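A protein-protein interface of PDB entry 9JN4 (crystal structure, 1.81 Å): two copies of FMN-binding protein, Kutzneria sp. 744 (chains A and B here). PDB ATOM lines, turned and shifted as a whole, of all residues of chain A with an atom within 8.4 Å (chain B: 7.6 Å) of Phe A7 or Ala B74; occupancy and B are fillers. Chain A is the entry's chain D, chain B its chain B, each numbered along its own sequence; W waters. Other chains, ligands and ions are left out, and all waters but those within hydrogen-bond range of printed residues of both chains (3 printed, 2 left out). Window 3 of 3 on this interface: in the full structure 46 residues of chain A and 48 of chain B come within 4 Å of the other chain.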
ATOM      1  N   ALA A   5      -7.599   3.988  -7.401  1.00  0.00           N
ATOM      2  CA  ALA A   5      -9.060   3.714  -7.261  1.00  0.00           C
ATOM      3  C   ALA A   5      -9.480   3.641  -5.779  1.00  0.00           C
ATOM      4  O   ALA A   5      -8.640   3.612  -4.820  1.00  0.00           O
ATOM      5  CB  ALA A   5      -9.485   2.484  -8.045  1.00  0.00           C
ATOM      6  N   MET A   6     -10.781   3.782  -5.597  1.00  0.00           N
ATOM      7  CA  MET A   6     -11.398   3.870  -4.259  1.00  0.00           C
ATOM      8  C   MET A   6     -12.345   2.684  -4.171  1.00  0.00           C
ATOM      9  O   MET A   6     -13.030   2.409  -5.170  1.00  0.00           O
ATOM     10  CB  MET A   6     -12.158   5.188  -4.148  1.00  0.00           C
ATOM     11  CG  MET A   6     -12.955   5.359  -2.894  1.00  0.00           C
ATOM     12  SD  MET A   6     -13.969   6.849  -3.049  1.00  0.00           S
ATOM     13  CE  MET A   6     -14.546   6.916  -1.358  1.00  0.00           C
ATOM     14  N   PHE A   7     -12.387   2.024  -3.025  1.00  0.00           N
ATOM     15  CA  PHE A   7     -13.286   0.871  -2.818  1.00  0.00           C
ATOM     16  C   PHE A   7     -14.659   1.398  -2.422  1.00  0.00           C
ATOM     17  O   PHE A   7     -14.765   2.061  -1.382  1.00  0.00           O
ATOM     18  CB  PHE A   7     -12.794  -0.022  -1.686  1.00  0.00           C
ATOM     19  CG  PHE A   7     -13.671  -1.220  -1.518  1.00  0.00           C
ATOM     20  CD1 PHE A   7     -13.837  -2.093  -2.578  1.00  0.00           C
ATOM     21  CD2 PHE A   7     -14.358  -1.450  -0.341  1.00  0.00           C
ATOM     22  CE1 PHE A   7     -14.640  -3.215  -2.438  1.00  0.00           C
ATOM     23  CE2 PHE A   7     -15.174  -2.561  -0.213  1.00  0.00           C
ATOM     24  CZ  PHE A   7     -15.308  -3.439  -1.260  1.00  0.00           C
ATOM     25  N   VAL A   8     -15.677   1.152  -3.225  1.00  0.00           N
ATOM     26  CA  VAL A   8     -17.059   1.571  -2.884  1.00  0.00           C
ATOM     27  C   VAL A   8     -17.961   0.378  -3.105  1.00  0.00           C
ATOM     28  O   VAL A   8     -18.157  -0.014  -4.260  1.00  0.00           O
ATOM     29  CB  VAL A   8     -17.534   2.759  -3.731  1.00  0.00           C
ATOM     30  CG1 VAL A   8     -18.928   3.168  -3.320  1.00  0.00           C
ATOM     31  CG2 VAL A   8     -16.553   3.924  -3.659  1.00  0.00           C
ATOM     32  N   PRO A   9     -18.534  -0.196  -2.030  1.00  0.00           N
ATOM     33  CA  PRO A   9     -19.513  -1.272  -2.186  1.00  0.00           C
ATOM     34  C   PRO A   9     -20.683  -0.839  -3.065  1.00  0.00           C
ATOM     35  O   PRO A   9     -21.147   0.289  -2.925  1.00  0.00           O
ATOM     36  CB  PRO A   9     -19.987  -1.560  -0.752  1.00  0.00           C
ATOM     37  CG  PRO A   9     -18.820  -1.100   0.127  1.00  0.00           C
ATOM     38  CD  PRO A   9     -18.255   0.096  -0.614  1.00  0.00           C
ATOM     39  N   GLY A  10     -21.197  -1.777  -3.871  1.00  0.00           N
ATOM     40  CA  GLY A  10     -22.268  -1.527  -4.858  1.00  0.00           C
ATOM     41  C   GLY A  10     -23.382  -0.634  -4.319  1.00  0.00           C
ATOM     42  O   GLY A  10     -23.713   0.363  -4.954  1.00  0.00           O
ATOM     43  N   TYR A  12     -23.530   1.648  -2.167  1.00  0.00           N
ATOM     44  CA  TYR A  12     -23.116   3.003  -1.712  1.00  0.00           C
ATOM     45  C   TYR A  12     -22.738   3.887  -2.923  1.00  0.00           C
ATOM     46  O   TYR A  12     -22.260   5.031  -2.729  1.00  0.00           O
ATOM     47  CB  TYR A  12     -22.004   2.850  -0.668  1.00  0.00           C
ATOM     48  CG  TYR A  12     -22.386   2.050   0.556  1.00  0.00           C
ATOM     49  CD1 TYR A  12     -23.692   2.054   1.020  1.00  0.00           C
ATOM     50  CD2 TYR A  12     -21.463   1.304   1.279  1.00  0.00           C
ATOM     51  CE1 TYR A  12     -24.068   1.301   2.119  1.00  0.00           C
ATOM     52  CE2 TYR A  12     -21.823   0.551   2.390  1.00  0.00           C
ATOM     53  CZ  TYR A  12     -23.145   0.551   2.809  1.00  0.00           C
ATOM     54  OH  TYR A  12     -23.583  -0.141   3.916  1.00  0.00           O
ATOM     55  N   HIS A  13     -22.943   3.410  -4.159  1.00  0.00           N
ATOM     56  CA  HIS A  13     -22.699   4.223  -5.381  1.00  0.00           C
ATOM     57  C   HIS A  13     -23.710   5.363  -5.443  1.00  0.00           C
ATOM     58  O   HIS A  13     -24.881   5.156  -5.096  1.00  0.00           O
ATOM     59  CB  HIS A  13     -22.722   3.355  -6.640  1.00  0.00           C
ATOM     60  CG  HIS A  13     -21.542   2.465  -6.740  1.00  0.00           C
ATOM     61  ND1 HIS A  13     -20.858   2.287  -7.923  1.00  0.00           N
ATOM     62  CD2 HIS A  13     -20.869   1.765  -5.807  1.00  0.00           C
ATOM     63  CE1 HIS A  13     -19.820   1.497  -7.714  1.00  0.00           C
ATOM     64  NE2 HIS A  13     -19.807   1.167  -6.424  1.00  0.00           N
ATOM     65  N   PHE A 114     -21.760   8.163   5.911  1.00  0.00           N
ATOM     66  CA  PHE A 114     -20.835   9.207   5.481  1.00  0.00           C
ATOM     67  C   PHE A 114     -20.841   9.292   3.960  1.00  0.00           C
ATOM     68  O   PHE A 114     -21.317   8.357   3.199  1.00  0.00           O
ATOM     69  CB  PHE A 114     -19.442   8.959   6.044  1.00  0.00           C
ATOM     70  CG  PHE A 114     -18.610   7.935   5.336  1.00  0.00           C
ATOM     71  CD1 PHE A 114     -18.641   6.609   5.737  1.00  0.00           C
ATOM     72  CD2 PHE A 114     -17.688   8.311   4.362  1.00  0.00           C
ATOM     73  CE1 PHE A 114     -17.836   5.663   5.113  1.00  0.00           C
ATOM     74  CE2 PHE A 114     -16.920   7.354   3.724  1.00  0.00           C
ATOM     75  CZ  PHE A 114     -17.027   6.029   4.071  1.00  0.00           C
ATOM     76  N   SER A 116     -18.185  10.634   0.736  1.00  0.00           N
ATOM     77  CA  SER A 116     -16.846  11.082   0.285  1.00  0.00           C
ATOM     78  C   SER A 116     -16.741  11.060  -1.215  1.00  0.00           C
ATOM     79  O   SER A 116     -17.311  10.171  -1.857  1.00  0.00           O
ATOM     80  CB  SER A 116     -15.687  10.366   0.967  1.00  0.00           C
ATOM     81  OG  SER A 116     -15.706   8.972   0.773  1.00  0.00           O
ATOM     82  N   GLN A 118     -13.386  10.896  -3.814  1.00  0.00           N
ATOM     83  CA  GLN A 118     -11.950  10.755  -4.124  1.00  0.00           C
ATOM     84  C   GLN A 118     -11.696  10.976  -5.592  1.00  0.00           C
ATOM     85  O   GLN A 118     -12.265  10.217  -6.453  1.00  0.00           O
ATOM     86  CB  GLN A 118     -11.390   9.433  -3.671  1.00  0.00           C
ATOM     87  CG  GLN A 118     -11.358   9.306  -2.163  1.00  0.00           C
ATOM     88  CD  GLN A 118     -10.865   7.957  -1.719  1.00  0.00           C
ATOM     89  OE1 GLN A 118     -10.076   7.335  -2.394  1.00  0.00           O
ATOM     90  NE2 GLN A 118     -11.259   7.560  -0.528  1.00  0.00           N
ATOM     91  N   ARG A 120      -8.605  11.432  -8.457  1.00  0.00           N
ATOM     92  CA  ARG A 120      -7.185  11.111  -8.686  1.00  0.00           C
ATOM     93  C   ARG A 120      -6.790  11.631 -10.075  1.00  0.00           C
ATOM     94  O   ARG A 120      -7.642  11.560 -11.066  1.00  0.00           O
ATOM     95  CB  ARG A 120      -6.943   9.606  -8.540  1.00  0.00           C
ATOM     96  CG  ARG A 120      -7.197   9.080  -7.135  1.00  0.00           C
ATOM     97  CD  ARG A 120      -7.066   7.550  -7.125  1.00  0.00           C
ATOM     98  NE  ARG A 120      -6.792   7.134  -5.767  1.00  0.00           N
ATOM     99  CZ  ARG A 120      -7.670   7.098  -4.759  1.00  0.00           C
ATOM    100  NH1 ARG A 120      -8.963   7.414  -4.902  1.00  0.00           N
ATOM    101  NH2 ARG A 120      -7.209   6.682  -3.596  1.00  0.00           N
ATOM    102  N   ASP A 178     -14.424   8.684  -7.785  1.00  0.00           N
ATOM    103  CA  ASP A 178     -15.194   7.650  -7.036  1.00  0.00           C
ATOM    104  C   ASP A 178     -15.936   8.375  -5.897  1.00  0.00           C
ATOM    105  O   ASP A 178     -15.415   9.381  -5.441  1.00  0.00           O
ATOM    106  CB  ASP A 178     -14.227   6.542  -6.599  1.00  0.00           C
ATOM    107  CG  ASP A 178     -13.551   5.745  -7.731  1.00  0.00           C
ATOM    108  OD1 ASP A 178     -14.287   4.986  -8.391  1.00  0.00           O
ATOM    109  OD2 ASP A 178     -12.271   5.865  -7.946  1.00  0.00           O
ATOM    110  N   GLY A 179     -17.143   7.939  -5.563  1.00  0.00           N
ATOM    111  CA  GLY A 179     -18.009   8.518  -4.521  1.00  0.00           C
ATOM    112  C   GLY A 179     -18.619   7.444  -3.644  1.00  0.00           C
ATOM    113  O   GLY A 179     -19.213   6.509  -4.180  1.00  0.00           O
ATOM    114  N   MET A 180     -18.313   7.507  -2.357  1.00  0.00           N
ATOM    115  CA  MET A 180     -18.937   6.734  -1.269  1.00  0.00           C
ATOM    116  C   MET A 180     -20.188   7.488  -0.816  1.00  0.00           C
ATOM    117  O   MET A 180     -20.050   8.640  -0.262  1.00  0.00           O
ATOM    118  CB  MET A 180     -17.946   6.565  -0.105  1.00  0.00           C
ATOM    119  CG  MET A 180     -18.483   5.798   1.067  1.00  0.00           C
ATOM    120  SD  MET A 180     -18.589   4.009   0.768  1.00  0.00           S
ATOM    121  CE  MET A 180     -16.844   3.632   0.856  1.00  0.00           C
ATOM    122  N   PHE A 181     -21.374   6.918  -1.035  1.00  0.00           N
ATOM    123  CA  PHE A 181     -22.597   7.480  -0.411  1.00  0.00           C
ATOM    124  C   PHE A 181     -23.184   6.425   0.520  1.00  0.00           C
ATOM    125  O   PHE A 181     -24.100   5.674   0.156  1.00  0.00           O
ATOM    126  CB  PHE A 181     -23.564   8.010  -1.461  1.00  0.00           C
ATOM    127  CG  PHE A 181     -22.985   9.202  -2.161  1.00  0.00           C
ATOM    128  CD1 PHE A 181     -21.987   9.049  -3.096  1.00  0.00           C
ATOM    129  CD2 PHE A 181     -23.357  10.480  -1.790  1.00  0.00           C
ATOM    130  CE1 PHE A 181     -21.410  10.160  -3.701  1.00  0.00           C
ATOM    131  CE2 PHE A 181     -22.789  11.587  -2.399  1.00  0.00           C
ATOM    132  CZ  PHE A 181     -21.828  11.421  -3.367  1.00  0.00           C
ATOM    133  N   HIS B  43      -3.730   5.170  -1.332  1.00  0.00           N
ATOM    134  CA  HIS B  43      -5.008   4.531  -0.940  1.00  0.00           C
ATOM    135  C   HIS B  43      -5.570   5.339   0.228  1.00  0.00           C
ATOM    136  O   HIS B  43      -4.765   5.740   1.077  1.00  0.00           O
ATOM    137  CB  HIS B  43      -4.837   3.081  -0.447  1.00  0.00           C
ATOM    138  CG  HIS B  43      -4.168   2.193  -1.419  1.00  0.00           C
ATOM    139  ND1 HIS B  43      -4.878   1.369  -2.245  1.00  0.00           N
ATOM    140  CD2 HIS B  43      -2.867   1.944  -1.636  1.00  0.00           C
ATOM    141  CE1 HIS B  43      -4.031   0.670  -2.969  1.00  0.00           C
ATOM    142  NE2 HIS B  43      -2.805   1.009  -2.625  1.00  0.00           N
ATOM    143  N   ILE B  44      -6.846   5.695   0.171  1.00  0.00           N
ATOM    144  CA  ILE B  44      -7.526   6.444   1.268  1.00  0.00           C
ATOM    145  C   ILE B  44      -8.792   5.677   1.650  1.00  0.00           C
ATOM    146  O   ILE B  44      -9.648   5.382   0.742  1.00  0.00           O
ATOM    147  CB  ILE B  44      -7.899   7.853   0.786  1.00  0.00           C
ATOM    148  CG1 ILE B  44      -6.727   8.643   0.194  1.00  0.00           C
ATOM    149  CG2 ILE B  44      -8.584   8.573   1.936  1.00  0.00           C
ATOM    150  CD1 ILE B  44      -5.899   9.282   1.270  1.00  0.00           C
ATOM    151  N   THR B  45      -8.935   5.320   2.922  1.00  0.00           N
ATOM    152  CA  THR B  45     -10.162   4.654   3.395  1.00  0.00           C
ATOM    153  C   THR B  45     -10.661   5.365   4.646  1.00  0.00           C
ATOM    154  O   THR B  45      -9.791   5.635   5.488  1.00  0.00           O
ATOM    155  CB  THR B  45      -9.921   3.167   3.673  1.00  0.00           C
ATOM    156  OG1 THR B  45      -9.460   2.549   2.469  1.00  0.00           O
ATOM    157  CG2 THR B  45     -11.195   2.504   4.147  1.00  0.00           C
ATOM    158  N   MET B  71     -11.386  -2.154   9.229  1.00  0.00           N
ATOM    159  CA  MET B  71     -11.792  -1.835   7.855  1.00  0.00           C
ATOM    160  C   MET B  71     -12.292  -3.138   7.232  1.00  0.00           C
ATOM    161  O   MET B  71     -12.360  -4.169   7.933  1.00  0.00           O
ATOM    162  CB  MET B  71     -10.631  -1.225   7.061  1.00  0.00           C
ATOM    163  CG  MET B  71      -9.553  -2.191   6.725  1.00  0.00           C
ATOM    164  SD  MET B  71      -8.404  -1.385   5.548  1.00  0.00           S
ATOM    165  CE  MET B  71      -7.255  -0.835   6.772  1.00  0.00           C
ATOM    166  N   ASN B  72     -12.732  -3.063   5.993  1.00  0.00           N
ATOM    167  CA  ASN B  72     -13.270  -4.236   5.263  1.00  0.00           C
ATOM    168  C   ASN B  72     -12.083  -5.016   4.679  1.00  0.00           C
ATOM    169  O   ASN B  72     -11.282  -4.402   3.981  1.00  0.00           O
ATOM    170  CB  ASN B  72     -14.284  -3.713   4.260  1.00  0.00           C
ATOM    171  CG  ASN B  72     -14.978  -4.800   3.498  1.00  0.00           C
ATOM    172  OD1 ASN B  72     -14.738  -5.979   3.727  1.00  0.00           O
ATOM    173  ND2 ASN B  72     -15.910  -4.367   2.681  1.00  0.00           N
ATOM    174  N   ARG B  73     -11.981  -6.330   4.926  1.00  0.00           N
ATOM    175  CA  ARG B  73     -10.912  -7.151   4.288  1.00  0.00           C
ATOM    176  C   ARG B  73     -11.036  -7.172   2.767  1.00  0.00           C
ATOM    177  O   ARG B  73     -10.002  -7.340   2.111  1.00  0.00           O
ATOM    178  CB  ARG B  73     -10.940  -8.573   4.863  1.00  0.00           C
ATOM    179  CG  ARG B  73     -10.273  -8.661   6.222  1.00  0.00           C
ATOM    180  CD  ARG B  73     -10.379 -10.077   6.796  1.00  0.00           C
ATOM    181  NE  ARG B  73      -9.688 -10.047   8.050  1.00  0.00           N
ATOM    182  CZ  ARG B  73      -8.496 -10.529   8.302  1.00  0.00           C
ATOM    183  NH1 ARG B  73      -7.811 -11.196   7.380  1.00  0.00           N
ATOM    184  NH2 ARG B  73      -8.003 -10.383   9.520  1.00  0.00           N
ATOM    185  N   ALA B  74     -12.247  -7.024   2.249  1.00  0.00           N
ATOM    186  CA  ALA B  74     -12.595  -7.050   0.819  1.00  0.00           C
ATOM    187  C   ALA B  74     -12.069  -5.787   0.137  1.00  0.00           C
ATOM    188  O   ALA B  74     -12.112  -5.752  -1.101  1.00  0.00           O
ATOM    189  CB  ALA B  74     -14.089  -7.177   0.650  1.00  0.00           C
ATOM    190  N   ASN B  75     -11.746  -4.754   0.924  1.00  0.00           N
ATOM    191  CA  ASN B  75     -11.180  -3.468   0.441  1.00  0.00           C
ATOM    192  C   ASN B  75      -9.735  -3.727  -0.012  1.00  0.00           C
ATOM    193  O   ASN B  75      -8.892  -4.162   0.777  1.00  0.00           O
ATOM    194  CB  ASN B  75     -11.349  -2.399   1.528  1.00  0.00           C
ATOM    195  CG  ASN B  75     -10.848  -1.041   1.101  1.00  0.00           C
ATOM    196  OD1 ASN B  75     -10.118  -0.913   0.104  1.00  0.00           O
ATOM    197  ND2 ASN B  75     -11.225  -0.043   1.871  1.00  0.00           N
ATOM    198  N   PRO B  76      -9.356  -3.446  -1.286  1.00  0.00           N
ATOM    199  CA  PRO B  76      -7.977  -3.647  -1.752  1.00  0.00           C
ATOM    200  C   PRO B  76      -6.925  -3.007  -0.852  1.00  0.00           C
ATOM    201  O   PRO B  76      -5.757  -3.420  -0.788  1.00  0.00           O
ATOM    202  CB  PRO B  76      -7.944  -2.931  -3.094  1.00  0.00           C
ATOM    203  CG  PRO B  76      -9.366  -3.043  -3.610  1.00  0.00           C
ATOM    204  CD  PRO B  76     -10.245  -3.013  -2.371  1.00  0.00           C
ATOM    205  N   HIS B  77      -7.361  -1.966  -0.152  1.00  0.00           N
ATOM    206  CA  HIS B  77      -6.472  -1.218   0.748  1.00  0.00           C
ATOM    207  C   HIS B  77      -5.950  -2.184   1.826  1.00  0.00           C
ATOM    208  O   HIS B  77      -4.758  -2.121   2.183  1.00  0.00           O
ATOM    209  CB  HIS B  77      -7.250  -0.046   1.343  1.00  0.00           C
ATOM    210  CG  HIS B  77      -6.332   0.920   1.975  1.00  0.00           C
ATOM    211  ND1 HIS B  77      -6.777   2.103   2.525  1.00  0.00           N
ATOM    212  CD2 HIS B  77      -4.999   0.886   2.142  1.00  0.00           C
ATOM    213  CE1 HIS B  77      -5.747   2.744   3.009  1.00  0.00           C
ATOM    214  NE2 HIS B  77      -4.648   2.056   2.727  1.00  0.00           N
ATOM    215  N   TRP B  78      -6.787  -3.113   2.271  1.00  0.00           N
ATOM    216  CA  TRP B  78      -6.357  -4.127   3.273  1.00  0.00           C
ATOM    217  C   TRP B  78      -5.155  -4.966   2.773  1.00  0.00           C
ATOM    218  O   TRP B  78      -4.130  -4.975   3.477  1.00  0.00           O
ATOM    219  CB  TRP B  78      -7.554  -4.964   3.706  1.00  0.00           C
ATOM    220  CG  TRP B  78      -7.218  -6.048   4.673  1.00  0.00           C
ATOM    221  CD1 TRP B  78      -7.068  -7.367   4.369  1.00  0.00           C
ATOM    222  CD2 TRP B  78      -6.923  -5.912   6.078  1.00  0.00           C
ATOM    223  NE1 TRP B  78      -6.683  -8.055   5.480  1.00  0.00           N
ATOM    224  CE2 TRP B  78      -6.606  -7.200   6.547  1.00  0.00           C
ATOM    225  CE3 TRP B  78      -6.921  -4.849   7.003  1.00  0.00           C
ATOM    226  CZ2 TRP B  78      -6.339  -7.449   7.894  1.00  0.00           C
ATOM    227  CZ3 TRP B  78      -6.625  -5.086   8.320  1.00  0.00           C
ATOM    228  CH2 TRP B  78      -6.354  -6.374   8.765  1.00  0.00           C
ATOM    229  N   ALA B  79      -5.246  -5.623   1.599  1.00  0.00           N
ATOM    230  CA  ALA B  79      -4.124  -6.365   0.979  1.00  0.00           C
ATOM    231  C   ALA B  79      -2.929  -5.425   0.710  1.00  0.00           C
ATOM    232  O   ALA B  79      -1.783  -5.881   0.891  1.00  0.00           O
ATOM    233  CB  ALA B  79      -4.592  -7.080  -0.280  1.00  0.00           C
ATOM    234  N   PRO B 165     -15.835 -12.523   9.890  1.00  0.00           N
ATOM    235  CA  PRO B 165     -14.688 -12.729   9.001  1.00  0.00           C
ATOM    236  C   PRO B 165     -14.292 -11.542   8.076  1.00  0.00           C
ATOM    237  O   PRO B 165     -13.101 -11.448   7.707  1.00  0.00           O
ATOM    238  CB  PRO B 165     -15.105 -13.959   8.157  1.00  0.00           C
ATOM    239  CG  PRO B 165     -16.158 -14.670   8.994  1.00  0.00           C
ATOM    240  CD  PRO B 165     -16.859 -13.575   9.783  1.00  0.00           C
ATOM    241  N   GLY B 166     -15.239 -10.652   7.769  1.00  0.00           N
ATOM    242  CA  GLY B 166     -15.081  -9.498   6.861  1.00  0.00           C
ATOM    243  C   GLY B 166     -14.291  -8.378   7.550  1.00  0.00           C
ATOM    244  O   GLY B 166     -13.721  -7.544   6.861  1.00  0.00           O
ATOM    245  N   VAL B 167     -14.209  -8.389   8.886  1.00  0.00           N
ATOM    246  CA  VAL B 167     -13.442  -7.338   9.643  1.00  0.00           C
ATOM    247  C   VAL B 167     -11.931  -7.507   9.476  1.00  0.00           C
ATOM    248  O   VAL B 167     -11.407  -8.605   9.784  1.00  0.00           O
ATOM    249  CB  VAL B 167     -13.812  -7.369  11.132  1.00  0.00           C
ATOM    250  CG1 VAL B 167     -13.075  -6.326  11.940  1.00  0.00           C
ATOM    251  CG2 VAL B 167     -15.312  -7.246  11.284  1.00  0.00           C
ATOM    252  N   GLY B 168     -11.245  -6.422   9.084  1.00  0.00           N
ATOM    253  CA  GLY B 168      -9.780  -6.283   9.091  1.00  0.00           C
ATOM    254  C   GLY B 168      -9.381  -5.391  10.236  1.00  0.00           C
ATOM    255  O   GLY B 168      -9.414  -4.127  10.067  1.00  0.00           O
HETATM  256  O   HOH W   1     -10.747   3.324  -0.304  1.00  0.00           O
HETATM  257  O   HOH W   2      -6.179   3.346  -4.686  1.00  0.00           O
HETATM  258  O   HOH W   3      -8.527   4.529  -2.098  1.00  0.00           O
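The side-chain amide nitrogen (NE2) of Gln A118 sits at hydrogen-bond distance from the backbone carbonyl oxygen (O) of Ile B44, 3.0 Å away.
OD1 of Asn B75 sits close to N of His B77, 3.0 Å away.
OE1 of Gln A118 is in hydrogen-bond range of NH1 of Arg A120 (2.7 Å).
N of Asp A178 sits at hydrogen-bond distance from O of Gln A118, 3.0 Å away.
The side-chain amide oxygen of Asn B72 is in hydrogen-bond range of the backbone NH of Ala B74 (3.1 Å).
The side-chain amide nitrogen (NE2) of Gln A118 lies close to the side-chain sulfur (SD) of Met A6 (3.8 Å).
OG1 of Thr B45 sits at hydrogen-bond distance from ND2 of Asn B75, at 3.2 Å.
Among the printed residues, merely in contact across the chains: Phe A7 with Asn B75 (3.3 Å), Phe A7 with Asn B72 (3.5 Å), Phe A7 with Pro B76 (3.7 Å), Phe A7 with Ala B74 (3.8 Å) and Arg A120 with Ile B44 (3.9 Å).
Printed residues of chain B within 4 Å of Phe A7: Asn B72 (3.5 Å), Ala B74 (3.8 Å), Asn B75 (3.3 Å) and Pro B76 (3.7 Å).
Of the printed residues of chain B, Gln A118 touches Ile B44.
Printed residues of chain B within 4 Å of Arg A120: Ile B44.
Of the printed residues of chain A, Asn B72 touches Phe A7 (3.5 Å).
Ala B74 touches just one residue of chain A: Phe A7 (3.8 Å).
Of chain A, only Phe A7 comes within 4 Å of Asn B75.
Of the printed residues of chain A, Pro B76 touches Phe A7 (3.7 Å).
The nearest residue of chain A that does not touch Ala B74 is Pro A9 (7.7 Å).
The nearest printed residue of chain B that does not touch Gln A118 is Thr B45 (4.7 Å).
Along chain B the printed residues that touch a printed residue of chain A span positions 44 to 76.
Among the printed residues, no Asp or Glu carboxylate lies within 4 Å of a Lys or Arg side-chain nitrogen of the other chain.
No position is printed for both chains.
Water W2 bridges O of Ala A5 (2.5 Å) and ND1 of His B43 (3.4 Å).
Water W1 lies within hydrogen-bond range of the backbone carbonyl oxygen of Ile B44, the side-chain hydroxyl of Thr B45 and the backbone NH of Phe A7.
Water W3 lies within hydrogen-bond range of the backbone carbonyl oxygen of Ala A5 (2.9 Å), the guanidinium group of Arg A120 (2.9 Å), the backbone NH of Ile B44 (3.1 Å) and the side-chain amide oxygen of Gln A118 (3.2 Å).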
